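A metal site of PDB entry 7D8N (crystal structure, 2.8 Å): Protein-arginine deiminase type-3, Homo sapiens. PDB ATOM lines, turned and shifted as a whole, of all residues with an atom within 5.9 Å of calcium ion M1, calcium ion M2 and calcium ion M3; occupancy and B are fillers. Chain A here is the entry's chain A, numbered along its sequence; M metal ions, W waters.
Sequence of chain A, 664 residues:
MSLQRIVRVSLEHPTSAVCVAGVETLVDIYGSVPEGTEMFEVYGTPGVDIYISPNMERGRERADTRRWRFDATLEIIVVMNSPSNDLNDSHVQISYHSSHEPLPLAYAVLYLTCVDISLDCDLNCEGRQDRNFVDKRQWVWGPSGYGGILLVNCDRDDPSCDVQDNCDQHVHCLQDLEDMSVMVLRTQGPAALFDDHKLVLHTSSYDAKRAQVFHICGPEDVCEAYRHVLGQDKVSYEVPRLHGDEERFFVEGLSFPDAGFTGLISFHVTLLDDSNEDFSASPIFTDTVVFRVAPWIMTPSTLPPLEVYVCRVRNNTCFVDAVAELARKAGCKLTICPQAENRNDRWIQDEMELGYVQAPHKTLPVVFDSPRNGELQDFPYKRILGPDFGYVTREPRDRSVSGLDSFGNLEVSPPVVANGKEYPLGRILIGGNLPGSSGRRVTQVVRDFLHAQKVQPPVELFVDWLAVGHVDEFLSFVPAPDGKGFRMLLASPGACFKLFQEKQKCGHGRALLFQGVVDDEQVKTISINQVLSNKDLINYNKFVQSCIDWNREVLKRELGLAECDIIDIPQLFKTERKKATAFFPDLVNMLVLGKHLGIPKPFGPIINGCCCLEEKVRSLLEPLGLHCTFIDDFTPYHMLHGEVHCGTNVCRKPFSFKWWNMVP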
ATOM      1  N   ASN A 153     -14.216 -24.669  20.794  1.00  0.00           N
ATOM      2  CA  ASN A 153     -14.960 -25.861  20.399  1.00  0.00           C
ATOM      3  C   ASN A 153     -14.404 -27.085  21.126  1.00  0.00           C
ATOM      4  O   ASN A 153     -13.764 -27.969  20.556  1.00  0.00           O
ATOM      5  CB  ASN A 153     -14.890 -26.030  18.882  1.00  0.00           C
ATOM      6  CG  ASN A 153     -15.804 -27.112  18.372  1.00  0.00           C
ATOM      7  OD1 ASN A 153     -16.642 -27.634  19.116  1.00  0.00           O
ATOM      8  ND2 ASN A 153     -15.662 -27.466  17.106  1.00  0.00           N
ATOM      9  N   CYS A 154     -14.681 -27.132  22.435  1.00  0.00           N
ATOM     10  CA  CYS A 154     -14.080 -28.107  23.331  1.00  0.00           C
ATOM     11  C   CYS A 154     -15.089 -29.124  23.870  1.00  0.00           C
ATOM     12  O   CYS A 154     -14.899 -29.634  24.978  1.00  0.00           O
ATOM     13  CB  CYS A 154     -13.391 -27.387  24.492  1.00  0.00           C
ATOM     14  SG  CYS A 154     -14.494 -26.284  25.417  1.00  0.00           S
ATOM     15  N   ASP A 155     -16.150 -29.441  23.121  1.00  0.00           N
ATOM     16  CA  ASP A 155     -17.272 -30.156  23.702  1.00  0.00           C
ATOM     17  C   ASP A 155     -17.535 -31.554  23.151  1.00  0.00           C
ATOM     18  O   ASP A 155     -18.400 -32.241  23.695  1.00  0.00           O
ATOM     19  CB  ASP A 155     -18.562 -29.323  23.583  1.00  0.00           C
ATOM     20  CG  ASP A 155     -19.084 -29.232  22.163  1.00  0.00           C
ATOM     21  OD1 ASP A 155     -18.266 -29.057  21.233  1.00  0.00           O
ATOM     22  OD2 ASP A 155     -20.313 -29.323  21.982  1.00  0.00           O
ATOM     23  N   ARG A 156     -16.824 -32.016  22.130  1.00  0.00           N
ATOM     24  CA  ARG A 156     -16.933 -33.408  21.661  1.00  0.00           C
ATOM     25  C   ARG A 156     -18.368 -33.763  21.251  1.00  0.00           C
ATOM     26  O   ARG A 156     -19.059 -34.543  21.900  1.00  0.00           O
ATOM     27  CB  ARG A 156     -16.410 -34.385  22.727  1.00  0.00           C
ATOM     28  CG  ARG A 156     -16.348 -35.832  22.263  1.00  0.00           C
ATOM     29  CD  ARG A 156     -16.509 -36.767  23.431  1.00  0.00           C
ATOM     30  NE  ARG A 156     -15.224 -37.178  23.981  1.00  0.00           N
ATOM     31  CZ  ARG A 156     -15.065 -37.719  25.186  1.00  0.00           C
ATOM     32  NH1 ARG A 156     -16.109 -37.904  25.970  1.00  0.00           N
ATOM     33  NH2 ARG A 156     -13.861 -38.066  25.602  1.00  0.00           N
ATOM     34  N   ASP A 157     -18.802 -33.144  20.157  1.00  0.00           N
ATOM     35  CA  ASP A 157     -20.109 -33.466  19.594  1.00  0.00           C
ATOM     36  C   ASP A 157     -20.108 -34.775  18.826  1.00  0.00           C
ATOM     37  O   ASP A 157     -21.167 -35.401  18.678  1.00  0.00           O
ATOM     38  CB  ASP A 157     -20.585 -32.352  18.648  1.00  0.00           C
ATOM     39  CG  ASP A 157     -21.047 -31.121  19.396  1.00  0.00           C
ATOM     40  OD1 ASP A 157     -21.680 -31.265  20.467  1.00  0.00           O
ATOM     41  OD2 ASP A 157     -20.781 -30.008  18.904  1.00  0.00           O
ATOM     42  N   GLN A 164     -11.941 -34.311  21.973  1.00  0.00           N
ATOM     43  CA  GLN A 164     -12.600 -33.041  21.695  1.00  0.00           C
ATOM     44  C   GLN A 164     -12.637 -32.767  20.200  1.00  0.00           C
ATOM     45  O   GLN A 164     -11.807 -33.253  19.423  1.00  0.00           O
ATOM     46  CB  GLN A 164     -11.903 -31.909  22.439  1.00  0.00           C
ATOM     47  CG  GLN A 164     -12.166 -31.921  23.941  1.00  0.00           C
ATOM     48  CD  GLN A 164     -11.088 -31.198  24.729  1.00  0.00           C
ATOM     49  OE1 GLN A 164     -11.347 -30.155  25.343  1.00  0.00           O
ATOM     50  NE2 GLN A 164      -9.885 -31.751  24.739  1.00  0.00           N
ATOM     51  N   ASP A 165     -13.618 -31.970  19.790  1.00  0.00           N
ATOM     52  CA  ASP A 165     -13.858 -31.744  18.365  1.00  0.00           C
ATOM     53  C   ASP A 165     -12.782 -30.907  17.706  1.00  0.00           C
ATOM     54  O   ASP A 165     -12.599 -31.006  16.493  1.00  0.00           O
ATOM     55  CB  ASP A 165     -15.228 -31.085  18.151  1.00  0.00           C
ATOM     56  CG  ASP A 165     -16.373 -31.985  18.562  1.00  0.00           C
ATOM     57  OD1 ASP A 165     -16.202 -33.222  18.542  1.00  0.00           O
ATOM     58  OD2 ASP A 165     -17.457 -31.456  18.899  1.00  0.00           O
ATOM     59  N   ASN A 166     -12.069 -30.078  18.466  1.00  0.00           N
ATOM     60  CA  ASN A 166     -11.081 -29.173  17.906  1.00  0.00           C
ATOM     61  C   ASN A 166      -9.660 -29.744  17.925  1.00  0.00           C
ATOM     62  O   ASN A 166      -8.695 -28.980  17.856  1.00  0.00           O
ATOM     63  CB  ASN A 166     -11.119 -27.830  18.636  1.00  0.00           C
ATOM     64  CG  ASN A 166     -10.817 -27.946  20.116  1.00  0.00           C
ATOM     65  OD1 ASN A 166     -10.554 -29.037  20.628  1.00  0.00           O
ATOM     66  ND2 ASN A 166     -10.855 -26.821  20.814  1.00  0.00           N
ATOM     67  N   CYS A 167      -9.510 -31.061  18.026  1.00  0.00           N
ATOM     68  CA  CYS A 167      -8.185 -31.660  18.032  1.00  0.00           C
ATOM     69  C   CYS A 167      -7.653 -31.955  16.637  1.00  0.00           C
ATOM     70  O   CYS A 167      -6.445 -31.922  16.434  1.00  0.00           O
ATOM     71  CB  CYS A 167      -8.191 -32.944  18.868  1.00  0.00           C
ATOM     72  SG  CYS A 167      -8.537 -32.666  20.612  1.00  0.00           S
ATOM     73  N   ASP A 168      -8.529 -32.256  15.690  1.00  0.00           N
ATOM     74  CA  ASP A 168      -8.119 -32.557  14.331  1.00  0.00           C
ATOM     75  C   ASP A 168      -8.255 -31.301  13.465  1.00  0.00           C
ATOM     76  O   ASP A 168      -8.463 -30.189  13.954  1.00  0.00           O
ATOM     77  CB  ASP A 168      -8.919 -33.731  13.776  1.00  0.00           C
ATOM     78  CG  ASP A 168     -10.418 -33.556  13.938  1.00  0.00           C
ATOM     79  OD1 ASP A 168     -10.857 -32.421  14.234  1.00  0.00           O
ATOM     80  OD2 ASP A 168     -11.145 -34.547  13.760  1.00  0.00           O
ATOM     81  N   GLN A 169      -8.120 -31.489  12.153  1.00  0.00           N
ATOM     82  CA  GLN A 169      -8.303 -30.424  11.175  1.00  0.00           C
ATOM     83  C   GLN A 169      -9.438 -30.757  10.215  1.00  0.00           C
ATOM     84  O   GLN A 169      -9.372 -30.449   9.019  1.00  0.00           O
ATOM     85  CB  GLN A 169      -7.005 -30.155  10.411  1.00  0.00           C
ATOM     86  CG  GLN A 169      -5.866 -29.670  11.285  1.00  0.00           C
ATOM     87  CD  GLN A 169      -4.657 -29.249  10.475  1.00  0.00           C
ATOM     88  OE1 GLN A 169      -4.729 -29.105   9.257  1.00  0.00           O
ATOM     89  NE2 GLN A 169      -3.529 -29.039  11.153  1.00  0.00           N
ATOM     90  N   HIS A 170     -10.487 -31.406  10.720  1.00  0.00           N
ATOM     91  CA  HIS A 170     -11.616 -31.805   9.896  1.00  0.00           C
ATOM     92  C   HIS A 170     -12.903 -31.588  10.672  1.00  0.00           C
ATOM     93  O   HIS A 170     -12.906 -31.493  11.902  1.00  0.00           O
ATOM     94  CB  HIS A 170     -11.526 -33.270   9.457  1.00  0.00           C
ATOM     95  CG  HIS A 170     -10.200 -33.651   8.870  1.00  0.00           C
ATOM     96  ND1 HIS A 170      -9.933 -33.558   7.513  1.00  0.00           N
ATOM     97  CD2 HIS A 170      -9.075 -34.125   9.440  1.00  0.00           C
ATOM     98  CE1 HIS A 170      -8.698 -33.957   7.289  1.00  0.00           C
ATOM     99  NE2 HIS A 170      -8.156 -34.314   8.438  1.00  0.00           N
ATOM    100  N   VAL A 171     -14.004 -31.487   9.933  1.00  0.00           N
ATOM    101  CA  VAL A 171     -15.344 -31.517  10.495  1.00  0.00           C
ATOM    102  C   VAL A 171     -15.883 -32.929  10.308  1.00  0.00           C
ATOM    103  O   VAL A 171     -15.966 -33.429   9.177  1.00  0.00           O
ATOM    104  CB  VAL A 171     -16.260 -30.474   9.818  1.00  0.00           C
ATOM    105  CG1 VAL A 171     -17.689 -30.627  10.310  1.00  0.00           C
ATOM    106  CG2 VAL A 171     -15.745 -29.068  10.088  1.00  0.00           C
ATOM    107  N   HIS A 172     -16.232 -33.581  11.411  1.00  0.00           N
ATOM    108  CA  HIS A 172     -16.688 -34.961  11.384  1.00  0.00           C
ATOM    109  C   HIS A 172     -18.145 -35.132  11.787  1.00  0.00           C
ATOM    110  O   HIS A 172     -18.623 -36.267  11.849  1.00  0.00           O
ATOM    111  CB  HIS A 172     -15.793 -35.828  12.277  1.00  0.00           C
ATOM    112  CG  HIS A 172     -14.443 -36.105  11.697  1.00  0.00           C
ATOM    113  ND1 HIS A 172     -14.214 -36.115  10.328  1.00  0.00           N
ATOM    114  CD2 HIS A 172     -13.256 -36.379  12.275  1.00  0.00           C
ATOM    115  CE1 HIS A 172     -12.935 -36.386  10.102  1.00  0.00           C
ATOM    116  NE2 HIS A 172     -12.332 -36.551  11.263  1.00  0.00           N
ATOM    117  N   GLN A 175     -23.411 -31.234  13.531  1.00  0.00           N
ATOM    118  CA  GLN A 175     -23.757 -30.502  14.744  1.00  0.00           C
ATOM    119  C   GLN A 175     -22.573 -29.708  15.290  1.00  0.00           C
ATOM    120  O   GLN A 175     -22.776 -28.770  16.059  1.00  0.00           O
ATOM    121  CB  GLN A 175     -24.313 -31.459  15.813  1.00  0.00           C
ATOM    122  CG  GLN A 175     -23.452 -32.684  16.100  1.00  0.00           C
ATOM    123  CD  GLN A 175     -23.797 -33.868  15.219  1.00  0.00           C
ATOM    124  OE1 GLN A 175     -23.723 -33.784  13.987  1.00  0.00           O
ATOM    125  NE2 GLN A 175     -24.181 -34.971  15.841  1.00  0.00           N
ATOM    126  N   ASP A 176     -21.348 -30.075  14.909  1.00  0.00           N
ATOM    127  CA  ASP A 176     -20.167 -29.343  15.365  1.00  0.00           C
ATOM    128  C   ASP A 176     -20.189 -27.893  14.895  1.00  0.00           C
ATOM    129  O   ASP A 176     -19.692 -27.017  15.594  1.00  0.00           O
ATOM    130  CB  ASP A 176     -18.903 -30.041  14.877  1.00  0.00           C
ATOM    131  CG  ASP A 176     -17.665 -29.582  15.628  1.00  0.00           C
ATOM    132  OD1 ASP A 176     -17.812 -28.972  16.699  1.00  0.00           O
ATOM    133  OD2 ASP A 176     -16.543 -29.833  15.133  1.00  0.00           O
ATOM    134  N   GLU A 178     -22.545 -25.892  14.896  1.00  0.00           N
ATOM    135  CA  GLU A 178     -23.359 -25.059  15.773  1.00  0.00           C
ATOM    136  C   GLU A 178     -22.514 -24.323  16.806  1.00  0.00           C
ATOM    137  O   GLU A 178     -22.985 -23.311  17.350  1.00  0.00           O
ATOM    138  CB  GLU A 178     -24.413 -25.914  16.473  1.00  0.00           C
ATOM    139  CG  GLU A 178     -25.364 -26.615  15.513  1.00  0.00           C
ATOM    140  CD  GLU A 178     -26.423 -27.440  16.244  1.00  0.00           C
ATOM    141  OE1 GLU A 178     -27.071 -28.273  15.570  1.00  0.00           O
ATOM    142  OE2 GLU A 178     -26.592 -27.257  17.467  1.00  0.00           O
ATOM    143  N   ASP A 179     -21.303 -24.800  17.101  1.00  0.00           N
ATOM    144  CA  ASP A 179     -20.399 -24.137  18.032  1.00  0.00           C
ATOM    145  C   ASP A 179     -19.556 -23.047  17.376  1.00  0.00           C
ATOM    146  O   ASP A 179     -19.072 -22.154  18.079  1.00  0.00           O
ATOM    147  CB  ASP A 179     -19.450 -25.143  18.685  1.00  0.00           C
ATOM    148  CG  ASP A 179     -20.176 -26.296  19.347  1.00  0.00           C
ATOM    149  OD1 ASP A 179     -21.141 -26.052  20.093  1.00  0.00           O
ATOM    150  OD2 ASP A 179     -19.764 -27.461  19.131  1.00  0.00           O
ATOM    151  N   PHE A 214     -12.391 -23.039   8.528  1.00  0.00           N
ATOM    152  CA  PHE A 214     -12.759 -23.930   7.425  1.00  0.00           C
ATOM    153  C   PHE A 214     -13.540 -23.137   6.392  1.00  0.00           C
ATOM    154  O   PHE A 214     -14.495 -22.442   6.730  1.00  0.00           O
ATOM    155  CB  PHE A 214     -13.615 -25.098   7.916  1.00  0.00           C
ATOM    156  CG  PHE A 214     -12.982 -25.906   9.019  1.00  0.00           C
ATOM    157  CD1 PHE A 214     -13.152 -25.538  10.338  1.00  0.00           C
ATOM    158  CD2 PHE A 214     -12.223 -27.021   8.722  1.00  0.00           C
ATOM    159  CE1 PHE A 214     -12.575 -26.276  11.352  1.00  0.00           C
ATOM    160  CE2 PHE A 214     -11.643 -27.766   9.724  1.00  0.00           C
ATOM    161  CZ  PHE A 214     -11.821 -27.394  11.047  1.00  0.00           C
ATOM    162  N   GLU A 252     -13.330 -21.593  14.620  1.00  0.00           N
ATOM    163  CA  GLU A 252     -13.380 -22.577  15.692  1.00  0.00           C
ATOM    164  C   GLU A 252     -12.257 -22.257  16.664  1.00  0.00           C
ATOM    165  O   GLU A 252     -11.082 -22.258  16.280  1.00  0.00           O
ATOM    166  CB  GLU A 252     -13.228 -23.985  15.112  1.00  0.00           C
ATOM    167  CG  GLU A 252     -12.847 -25.053  16.093  1.00  0.00           C
ATOM    168  CD  GLU A 252     -12.512 -26.362  15.399  1.00  0.00           C
ATOM    169  OE1 GLU A 252     -11.508 -26.395  14.649  1.00  0.00           O
ATOM    170  OE2 GLU A 252     -13.256 -27.338  15.573  1.00  0.00           O
ATOM    171  N   LYS A 362     -24.734 -19.807  20.814  1.00  0.00           N
ATOM    172  CA  LYS A 362     -24.711 -21.069  21.557  1.00  0.00           C
ATOM    173  C   LYS A 362     -24.120 -20.866  22.945  1.00  0.00           C
ATOM    174  O   LYS A 362     -23.183 -20.091  23.134  1.00  0.00           O
ATOM    175  CB  LYS A 362     -23.918 -22.136  20.797  1.00  0.00           C
ATOM    176  CG  LYS A 362     -23.920 -23.492  21.465  1.00  0.00           C
ATOM    177  CD  LYS A 362     -23.787 -24.602  20.441  1.00  0.00           C
ATOM    178  CE  LYS A 362     -25.144 -25.146  20.048  1.00  0.00           C
ATOM    179  NZ  LYS A 362     -25.911 -25.599  21.239  1.00  0.00           N
ATOM    180  N   LEU A 364     -22.564 -23.203  26.142  1.00  0.00           N
ATOM    181  CA  LEU A 364     -22.028 -24.517  26.471  1.00  0.00           C
ATOM    182  C   LEU A 364     -21.651 -24.561  27.948  1.00  0.00           C
ATOM    183  O   LEU A 364     -20.788 -23.772  28.375  1.00  0.00           O
ATOM    184  CB  LEU A 364     -20.804 -24.846  25.615  1.00  0.00           C
ATOM    185  CG  LEU A 364     -20.933 -24.880  24.098  1.00  0.00           C
ATOM    186  CD1 LEU A 364     -19.596 -25.257  23.501  1.00  0.00           C
ATOM    187  CD2 LEU A 364     -22.018 -25.839  23.660  1.00  0.00           C
ATOM    188  N   PRO A 387     -21.618 -34.165  24.025  1.00  0.00           N
ATOM    189  CA  PRO A 387     -22.183 -33.174  23.110  1.00  0.00           C
ATOM    190  C   PRO A 387     -22.793 -31.993  23.866  1.00  0.00           C
ATOM    191  O   PRO A 387     -23.565 -32.169  24.815  1.00  0.00           O
ATOM    192  CB  PRO A 387     -23.252 -33.970  22.345  1.00  0.00           C
ATOM    193  CG  PRO A 387     -23.531 -35.166  23.184  1.00  0.00           C
ATOM    194  CD  PRO A 387     -22.232 -35.494  23.846  1.00  0.00           C
ATOM    195  N   ASP A 388     -22.399 -30.786  23.453  1.00  0.00           N
ATOM    196  CA  ASP A 388     -22.819 -29.549  24.106  1.00  0.00           C
ATOM    197  C   ASP A 388     -22.433 -29.512  25.585  1.00  0.00           C
ATOM    198  O   ASP A 388     -23.151 -28.971  26.429  1.00  0.00           O
ATOM    199  CB  ASP A 388     -24.321 -29.312  23.939  1.00  0.00           C
ATOM    200  CG  ASP A 388     -24.651 -28.566  22.661  1.00  0.00           C
ATOM    201  OD1 ASP A 388     -23.824 -28.597  21.726  1.00  0.00           O
ATOM    202  OD2 ASP A 388     -25.727 -27.936  22.597  1.00  0.00           O
ATOM    203  N   PHE A 389     -21.283 -30.092  25.897  1.00  0.00           N
ATOM    204  CA  PHE A 389     -20.721 -29.999  27.244  1.00  0.00           C
ATOM    205  C   PHE A 389     -19.201 -30.048  27.085  1.00  0.00           C
ATOM    206  O   PHE A 389     -18.650 -31.110  26.785  1.00  0.00           O
ATOM    207  CB  PHE A 389     -21.236 -31.112  28.140  1.00  0.00           C
ATOM    208  CG  PHE A 389     -21.399 -30.702  29.579  1.00  0.00           C
ATOM    209  CD1 PHE A 389     -20.471 -29.879  30.202  1.00  0.00           C
ATOM    210  CD2 PHE A 389     -22.498 -31.125  30.313  1.00  0.00           C
ATOM    211  CE1 PHE A 389     -20.622 -29.509  31.533  1.00  0.00           C
ATOM    212  CE2 PHE A 389     -22.660 -30.746  31.635  1.00  0.00           C
ATOM    213  CZ  PHE A 389     -21.721 -29.934  32.243  1.00  0.00           C
HETATM  214 CA    CA M   1     -18.319 -29.278  18.941  1.00  0.00          CA
HETATM  215 CA    CA M   2     -13.127 -31.686  14.248  1.00  0.00          CA
HETATM  216 CA    CA M   3     -21.884 -28.532  20.300  1.00  0.00          CA
HETATM  217  O   HOH W   1     -14.111 -29.340  14.362  1.00  0.00           O
HETATM  218  O   HOH W   2     -23.633 -28.625  18.349  1.00  0.00           O
HETATM  219  O   HOH W   3     -11.798 -29.793  13.969  1.00  0.00           O
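Calcium ion M1 is bound by OD1 of Asp 155 (2.3 Å), OD1 of Asp 176 (2.3 Å), OD2 of Asp 179 (2.3 Å), OD2 of Asp 165 (2.3 Å), OD1 of Asn 153 (2.4 Å) and OD2 of Asp 157 (2.6 Å).
Of the 25 residues printed, 4 come within 4 Å of calcium ion M2.
Along chain A the residues within 4 Å of calcium ion M2 span positions 165 to 176.
Water W3 binds calcium ion M2, at 2.3 Å.
Calcium ion M2 is bound by the backbone carbonyl oxygen (O) of His 170 (2.4 Å).
OD1 of Asp 168 is bound to calcium ion M2 (2.4 Å).
O of Asp 165 binds calcium ion M2.
Water W1 binds calcium ion M2 (2.5 Å).
Calcium ion M2 has five donor atoms within binding distance.
Calcium ion M3 is bound by the side-chain carboxylate (OD2) of Asp 157 (2.3 Å), the side-chain carboxylate (OD1) of Asp 388 (2.4 Å), the side-chain carboxylate (OD2) of Asp 155 (2.4 Å), the side-chain carboxylate (OD1) of Asp 179 (2.6 Å), water W2 (2.6 Å), the side-chain carboxylate (OD2) of Asp 179 (2.6 Å) and the side-chain carboxylate (OD1) of Asp 157 (2.7 Å).
Within 4 Å of calcium ion M1: Asn 153, Asp 155, Asp 157, Asp 165, Asp 176 and Asp 179.
Water W3 bridges the side-chain carboxylate (OE2) of Glu 252 and the backbone carbonyl oxygen (O) of Asp 168.
Water W1 bridges the side-chain carboxylate (OE2) of Glu 252 (2.5 Å) and the side-chain carboxylate (OD2) of Asp 176 (2.6 Å).
Water W2 bridges O of Gln 175 (2.4 Å) and OE2 of Glu 178 (3.4 Å).
Within 4 Å of calcium ion M3: Asp 155, Asp 157, Asp 179 and Asp 388.
The nearest printed residue that does not touch calcium ion M3 is Leu 364 (4.3 Å).
OD2 of Asp 165 lies close to N of Arg 156 (3.3 Å).
The side-chain amide nitrogen (ND2) of Asn 153 sits at hydrogen-bond distance from the side-chain carboxylate (OE2) of Glu 252 (2.9 Å).
The side-chain amide nitrogen of Asn 166 sits close to the backbone carbonyl oxygen of Asn 153 (3.1 Å).
A ring nitrogen (NE2) of His 172 sits close to the side-chain carboxylate (OD2) of Asp 168 (3.4 Å).
OD2 of Asp 388 is in salt-bridge range of NZ of Lys 362 (2.7 Å).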
